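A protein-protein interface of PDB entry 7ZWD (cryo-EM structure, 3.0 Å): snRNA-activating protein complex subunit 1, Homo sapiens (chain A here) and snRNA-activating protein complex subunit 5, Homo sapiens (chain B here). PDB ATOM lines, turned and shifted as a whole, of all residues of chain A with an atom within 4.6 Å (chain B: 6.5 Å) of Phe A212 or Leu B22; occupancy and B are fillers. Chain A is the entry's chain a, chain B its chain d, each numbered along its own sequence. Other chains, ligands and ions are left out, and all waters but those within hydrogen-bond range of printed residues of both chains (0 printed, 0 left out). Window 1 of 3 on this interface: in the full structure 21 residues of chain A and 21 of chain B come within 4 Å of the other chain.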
ATOM      1  N   MET A 180      -4.376 -19.124  -6.906  1.00  0.00           N
ATOM      2  CA  MET A 180      -3.001 -18.746  -7.214  1.00  0.00           C
ATOM      3  C   MET A 180      -2.963 -17.486  -8.071  1.00  0.00           C
ATOM      4  O   MET A 180      -2.228 -16.541  -7.771  1.00  0.00           O
ATOM      5  CB  MET A 180      -2.284 -19.910  -7.907  1.00  0.00           C
ATOM      6  CG  MET A 180      -0.866 -19.613  -8.404  1.00  0.00           C
ATOM      7  SD  MET A 180      -0.735 -18.776 -10.001  1.00  0.00           S
ATOM      8  CE  MET A 180      -1.934 -19.690 -10.968  1.00  0.00           C
ATOM      9  N   HIS A 184      -1.663 -13.753  -7.220  1.00  0.00           N
ATOM     10  CA  HIS A 184      -0.634 -13.167  -8.077  1.00  0.00           C
ATOM     11  C   HIS A 184      -1.043 -11.787  -8.588  1.00  0.00           C
ATOM     12  O   HIS A 184      -0.255 -10.835  -8.529  1.00  0.00           O
ATOM     13  CB  HIS A 184      -0.323 -14.107  -9.242  1.00  0.00           C
ATOM     14  CG  HIS A 184       0.639 -15.201  -8.893  1.00  0.00           C
ATOM     15  ND1 HIS A 184       1.700 -15.543  -9.702  1.00  0.00           N
ATOM     16  CD2 HIS A 184       0.708 -16.019  -7.817  1.00  0.00           C
ATOM     17  CE1 HIS A 184       2.378 -16.530  -9.144  1.00  0.00           C
ATOM     18  NE2 HIS A 184       1.797 -16.838  -7.998  1.00  0.00           N
ATOM     19  N   LYS A 209       7.819 -14.074 -10.932  1.00  0.00           N
ATOM     20  CA  LYS A 209       7.770 -14.862 -12.154  1.00  0.00           C
ATOM     21  C   LYS A 209       6.340 -14.930 -12.673  1.00  0.00           C
ATOM     22  O   LYS A 209       5.387 -15.064 -11.900  1.00  0.00           O
ATOM     23  CB  LYS A 209       8.329 -16.271 -11.926  1.00  0.00           C
ATOM     24  CG  LYS A 209       7.436 -17.211 -11.131  1.00  0.00           C
ATOM     25  CD  LYS A 209       7.850 -18.659 -11.350  1.00  0.00           C
ATOM     26  CE  LYS A 209       7.745 -19.474 -10.071  1.00  0.00           C
ATOM     27  NZ  LYS A 209       7.986 -20.923 -10.320  1.00  0.00           N
ATOM     28  N   ASP A 210       6.198 -14.800 -13.991  1.00  0.00           N
ATOM     29  CA  ASP A 210       4.904 -14.867 -14.653  1.00  0.00           C
ATOM     30  C   ASP A 210       4.657 -16.235 -15.276  1.00  0.00           C
ATOM     31  O   ASP A 210       3.520 -16.549 -15.643  1.00  0.00           O
ATOM     32  CB  ASP A 210       4.810 -13.757 -15.707  1.00  0.00           C
ATOM     33  CG  ASP A 210       3.434 -13.649 -16.341  1.00  0.00           C
ATOM     34  OD1 ASP A 210       3.101 -14.475 -17.216  1.00  0.00           O
ATOM     35  OD2 ASP A 210       2.679 -12.731 -15.957  1.00  0.00           O
ATOM     36  N   ASP A 211       5.683 -17.078 -15.350  1.00  0.00           N
ATOM     37  CA  ASP A 211       5.576 -18.384 -15.981  1.00  0.00           C
ATOM     38  C   ASP A 211       5.209 -19.493 -15.007  1.00  0.00           C
ATOM     39  O   ASP A 211       5.150 -20.655 -15.416  1.00  0.00           O
ATOM     40  CB  ASP A 211       6.887 -18.727 -16.700  1.00  0.00           C
ATOM     41  CG  ASP A 211       8.092 -18.719 -15.772  1.00  0.00           C
ATOM     42  OD1 ASP A 211       8.036 -19.334 -14.686  1.00  0.00           O
ATOM     43  OD2 ASP A 211       9.108 -18.089 -16.135  1.00  0.00           O
ATOM     44  N   PHE A 212       4.969 -19.167 -13.734  1.00  0.00           N
ATOM     45  CA  PHE A 212       4.558 -20.187 -12.772  1.00  0.00           C
ATOM     46  C   PHE A 212       3.287 -20.888 -13.234  1.00  0.00           C
ATOM     47  O   PHE A 212       3.213 -22.123 -13.249  1.00  0.00           O
ATOM     48  CB  PHE A 212       4.350 -19.560 -11.395  1.00  0.00           C
ATOM     49  CG  PHE A 212       3.930 -20.544 -10.343  1.00  0.00           C
ATOM     50  CD1 PHE A 212       4.847 -21.422  -9.794  1.00  0.00           C
ATOM     51  CD2 PHE A 212       2.616 -20.597  -9.909  1.00  0.00           C
ATOM     52  CE1 PHE A 212       4.467 -22.332  -8.828  1.00  0.00           C
ATOM     53  CE2 PHE A 212       2.229 -21.506  -8.941  1.00  0.00           C
ATOM     54  CZ  PHE A 212       3.157 -22.374  -8.400  1.00  0.00           C
ATOM     55  N   PHE A 213       2.273 -20.107 -13.614  1.00  0.00           N
ATOM     56  CA  PHE A 213       1.082 -20.683 -14.224  1.00  0.00           C
ATOM     57  C   PHE A 213       1.451 -21.457 -15.484  1.00  0.00           C
ATOM     58  O   PHE A 213       1.024 -22.601 -15.672  1.00  0.00           O
ATOM     59  CB  PHE A 213       0.076 -19.575 -14.543  1.00  0.00           C
ATOM     60  CG  PHE A 213      -1.270 -20.075 -14.997  1.00  0.00           C
ATOM     61  CD1 PHE A 213      -2.158 -19.219 -15.627  1.00  0.00           C
ATOM     62  CD2 PHE A 213      -1.663 -21.384 -14.764  1.00  0.00           C
ATOM     63  CE1 PHE A 213      -3.400 -19.666 -16.043  1.00  0.00           C
ATOM     64  CE2 PHE A 213      -2.903 -21.836 -15.176  1.00  0.00           C
ATOM     65  CZ  PHE A 213      -3.772 -20.975 -15.814  1.00  0.00           C
ATOM     66  N   ASP A 214       2.269 -20.853 -16.348  1.00  0.00           N
ATOM     67  CA  ASP A 214       2.660 -21.516 -17.586  1.00  0.00           C
ATOM     68  C   ASP A 214       3.501 -22.758 -17.313  1.00  0.00           C
ATOM     69  O   ASP A 214       3.350 -23.777 -17.994  1.00  0.00           O
ATOM     70  CB  ASP A 214       3.413 -20.539 -18.490  1.00  0.00           C
ATOM     71  CG  ASP A 214       2.679 -19.224 -18.664  1.00  0.00           C
ATOM     72  OD1 ASP A 214       1.766 -19.161 -19.513  1.00  0.00           O
ATOM     73  OD2 ASP A 214       3.013 -18.253 -17.954  1.00  0.00           O
ATOM     74  N   ASN A 215       4.382 -22.701 -16.310  1.00  0.00           N
ATOM     75  CA  ASN A 215       5.210 -23.863 -16.000  1.00  0.00           C
ATOM     76  C   ASN A 215       4.366 -25.015 -15.470  1.00  0.00           C
ATOM     77  O   ASN A 215       4.509 -26.158 -15.925  1.00  0.00           O
ATOM     78  CB  ASN A 215       6.331 -23.542 -15.013  1.00  0.00           C
ATOM     79  CG  ASN A 215       7.291 -24.703 -14.821  1.00  0.00           C
ATOM     80  OD1 ASN A 215       7.464 -25.536 -15.712  1.00  0.00           O
ATOM     81  ND2 ASN A 215       7.925 -24.760 -13.655  1.00  0.00           N
ATOM     82  N   ILE A 216       3.485 -24.740 -14.506  1.00  0.00           N
ATOM     83  CA  ILE A 216       2.655 -25.807 -13.955  1.00  0.00           C
ATOM     84  C   ILE A 216       1.693 -26.329 -15.016  1.00  0.00           C
ATOM     85  O   ILE A 216       1.355 -27.520 -15.033  1.00  0.00           O
ATOM     86  CB  ILE A 216       1.922 -25.327 -12.686  1.00  0.00           C
ATOM     87  CG1 ILE A 216       1.442 -26.527 -11.867  1.00  0.00           C
ATOM     88  CG2 ILE A 216       0.760 -24.404 -13.028  1.00  0.00           C
ATOM     89  CD1 ILE A 216       1.314 -26.243 -10.388  1.00  0.00           C
ATOM     90  N   ARG B  17       8.602 -32.461 -10.366  1.00  0.00           N
ATOM     91  CA  ARG B  17       8.607 -31.267 -11.207  1.00  0.00           C
ATOM     92  C   ARG B  17       7.846 -30.126 -10.537  1.00  0.00           C
ATOM     93  O   ARG B  17       8.297 -28.970 -10.532  1.00  0.00           O
ATOM     94  CB  ARG B  17       8.012 -31.603 -12.574  1.00  0.00           C
ATOM     95  CG  ARG B  17       8.953 -32.388 -13.474  1.00  0.00           C
ATOM     96  CD  ARG B  17       8.260 -32.885 -14.733  1.00  0.00           C
ATOM     97  NE  ARG B  17       7.531 -34.130 -14.507  1.00  0.00           N
ATOM     98  CZ  ARG B  17       6.687 -34.669 -15.382  1.00  0.00           C
ATOM     99  NH1 ARG B  17       6.465 -34.071 -16.544  1.00  0.00           N
ATOM    100  NH2 ARG B  17       6.068 -35.806 -15.099  1.00  0.00           N
ATOM    101  N   LEU B  18       6.688 -30.442  -9.950  1.00  0.00           N
ATOM    102  CA  LEU B  18       5.939 -29.426  -9.212  1.00  0.00           C
ATOM    103  C   LEU B  18       6.737 -28.897  -8.027  1.00  0.00           C
ATOM    104  O   LEU B  18       6.719 -27.691  -7.748  1.00  0.00           O
ATOM    105  CB  LEU B  18       4.594 -29.981  -8.740  1.00  0.00           C
ATOM    106  CG  LEU B  18       3.735 -30.739  -9.747  1.00  0.00           C
ATOM    107  CD1 LEU B  18       2.435 -31.174  -9.106  1.00  0.00           C
ATOM    108  CD2 LEU B  18       3.459 -29.853 -10.945  1.00  0.00           C
ATOM    109  N   LYS B  19       7.437 -29.779  -7.312  1.00  0.00           N
ATOM    110  CA  LYS B  19       8.248 -29.328  -6.185  1.00  0.00           C
ATOM    111  C   LYS B  19       9.398 -28.453  -6.648  1.00  0.00           C
ATOM    112  O   LYS B  19       9.752 -27.490  -5.969  1.00  0.00           O
ATOM    113  CB  LYS B  19       8.780 -30.516  -5.390  1.00  0.00           C
ATOM    114  CG  LYS B  19       7.708 -31.384  -4.799  1.00  0.00           C
ATOM    115  CD  LYS B  19       8.290 -32.357  -3.811  1.00  0.00           C
ATOM    116  CE  LYS B  19       7.420 -33.580  -3.726  1.00  0.00           C
ATOM    117  NZ  LYS B  19       6.047 -33.345  -4.247  1.00  0.00           N
ATOM    118  N   ALA B  20       9.996 -28.770  -7.796  1.00  0.00           N
ATOM    119  CA  ALA B  20      11.045 -27.915  -8.339  1.00  0.00           C
ATOM    120  C   ALA B  20      10.507 -26.523  -8.639  1.00  0.00           C
ATOM    121  O   ALA B  20      11.120 -25.511  -8.273  1.00  0.00           O
ATOM    122  CB  ALA B  20      11.641 -28.547  -9.596  1.00  0.00           C
ATOM    123  N   ALA B  21       9.350 -26.455  -9.305  1.00  0.00           N
ATOM    124  CA  ALA B  21       8.752 -25.155  -9.603  1.00  0.00           C
ATOM    125  C   ALA B  21       8.448 -24.377  -8.326  1.00  0.00           C
ATOM    126  O   ALA B  21       8.791 -23.189  -8.210  1.00  0.00           O
ATOM    127  CB  ALA B  21       7.483 -25.341 -10.433  1.00  0.00           C
ATOM    128  N   LEU B  22       7.814 -25.032  -7.350  1.00  0.00           N
ATOM    129  CA  LEU B  22       7.448 -24.348  -6.114  1.00  0.00           C
ATOM    130  C   LEU B  22       8.677 -23.955  -5.302  1.00  0.00           C
ATOM    131  O   LEU B  22       8.663 -22.936  -4.607  1.00  0.00           O
ATOM    132  CB  LEU B  22       6.513 -25.228  -5.283  1.00  0.00           C
ATOM    133  CG  LEU B  22       5.010 -25.022  -5.481  1.00  0.00           C
ATOM    134  CD1 LEU B  22       4.536 -25.585  -6.808  1.00  0.00           C
ATOM    135  CD2 LEU B  22       4.238 -25.642  -4.324  1.00  0.00           C
ATOM    136  N   HIS B  23       9.754 -24.739  -5.383  1.00  0.00           N
ATOM    137  CA  HIS B  23      10.974 -24.394  -4.663  1.00  0.00           C
ATOM    138  C   HIS B  23      11.666 -23.195  -5.295  1.00  0.00           C
ATOM    139  O   HIS B  23      12.194 -22.336  -4.581  1.00  0.00           O
ATOM    140  CB  HIS B  23      11.918 -25.593  -4.609  1.00  0.00           C
ATOM    141  CG  HIS B  23      11.452 -26.691  -3.705  1.00  0.00           C
ATOM    142  ND1 HIS B  23      11.520 -28.022  -4.055  1.00  0.00           N
ATOM    143  CD2 HIS B  23      10.910 -26.655  -2.466  1.00  0.00           C
ATOM    144  CE1 HIS B  23      11.041 -28.759  -3.069  1.00  0.00           C
ATOM    145  NE2 HIS B  23      10.663 -27.954  -2.092  1.00  0.00           N
ATOM    146  N   ASP B  24      11.690 -23.123  -6.628  1.00  0.00           N
ATOM    147  CA  ASP B  24      12.191 -21.913  -7.275  1.00  0.00           C
ATOM    148  C   ASP B  24      11.354 -20.704  -6.875  1.00  0.00           C
ATOM    149  O   ASP B  24      11.890 -19.617  -6.611  1.00  0.00           O
ATOM    150  CB  ASP B  24      12.203 -22.084  -8.794  1.00  0.00           C
ATOM    151  CG  ASP B  24      12.876 -23.368  -9.232  1.00  0.00           C
ATOM    152  OD1 ASP B  24      13.818 -23.813  -8.543  1.00  0.00           O
ATOM    153  OD2 ASP B  24      12.462 -23.934 -10.266  1.00  0.00           O
ATOM    154  N   GLN B  25      10.029 -20.881  -6.824  1.00  0.00           N
ATOM    155  CA  GLN B  25       9.155 -19.801  -6.378  1.00  0.00           C
ATOM    156  C   GLN B  25       9.488 -19.379  -4.949  1.00  0.00           C
ATOM    157  O   GLN B  25       9.550 -18.185  -4.649  1.00  0.00           O
ATOM    158  CB  GLN B  25       7.692 -20.235  -6.492  1.00  0.00           C
ATOM    159  CG  GLN B  25       6.633 -19.166  -6.183  1.00  0.00           C
ATOM    160  CD  GLN B  25       6.876 -17.829  -6.863  1.00  0.00           C
ATOM    161  OE1 GLN B  25       7.746 -17.058  -6.464  1.00  0.00           O
ATOM    162  NE2 GLN B  25       6.094 -17.547  -7.899  1.00  0.00           N
ATOM    163  N   LEU B  26       9.735 -20.348  -4.064  1.00  0.00           N
ATOM    164  CA  LEU B  26      10.081 -20.029  -2.680  1.00  0.00           C
ATOM    165  C   LEU B  26      11.409 -19.287  -2.587  1.00  0.00           C
ATOM    166  O   LEU B  26      11.538 -18.326  -1.819  1.00  0.00           O
ATOM    167  CB  LEU B  26      10.139 -21.302  -1.837  1.00  0.00           C
ATOM    168  CG  LEU B  26       9.868 -21.103  -0.343  1.00  0.00           C
ATOM    169  CD1 LEU B  26       8.432 -20.666  -0.099  1.00  0.00           C
ATOM    170  CD2 LEU B  26      10.210 -22.354   0.454  1.00  0.00           C
ATOM    171  N   ASN B  27      12.417 -19.737  -3.337  1.00  0.00           N
ATOM    172  CA  ASN B  27      13.718 -19.075  -3.284  1.00  0.00           C
ATOM    173  C   ASN B  27      13.627 -17.639  -3.779  1.00  0.00           C
ATOM    174  O   ASN B  27      14.122 -16.717  -3.116  1.00  0.00           O
ATOM    175  CB  ASN B  27      14.753 -19.860  -4.091  1.00  0.00           C
ATOM    176  CG  ASN B  27      14.784 -21.331  -3.728  1.00  0.00           C
ATOM    177  OD1 ASN B  27      14.380 -21.723  -2.633  1.00  0.00           O
ATOM    178  ND2 ASN B  27      15.266 -22.157  -4.650  1.00  0.00           N
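The backbone carbonyl oxygen (O) of Ala B21 sits at hydrogen-bond distance from the side-chain amino group (NZ) of Lys A209.
Gln B25 touches Lys A209.
Leu B22 touches Phe A212.
Ala B21 touches Asn A215 (CB to ND2, 3.3 Å).
Leu B18 touches Ile A216.
Of the printed residues of chain B, Phe A212 touches Leu B22.
Leu B22 touches one residue of chain A.
Of the printed residues of chain B, Lys A209 touches Ala B21 (3.2 Å) and Gln B25 (3.3 Å).
Of the printed residues of chain A, Leu B18 touches Ile A216 (3.998 Å).
Of the printed residues of chain A, Gln B25 touches Lys A209.
Printed residues of chain B within 4 Å of Ile A216: Leu B18 (3.998 Å).
Asp A214 touches none of the printed residues of chain B.
His A184 touches none of the printed residues of chain B.
The nearest residue of chain B that does not touch Phe A212 is Gln B25 (4.4 Å).
The nearest printed residue of chain A that does not touch Gln B25 is His A184 (4.05 Å).
Of the 10 printed residues of chain A, 4 touch a printed residue of chain B.
Hydrophobic or aromatic side chains of chain A within 4 Å of the printed part of chain B: Phe A212 and Ile A216.
Of the 11 printed residues of chain B, 4 touch a printed residue of chain A.
Printed residues of chain B that touch a printed residue of chain A: Leu B18, Ala B21, Leu B22 and Gln B25.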
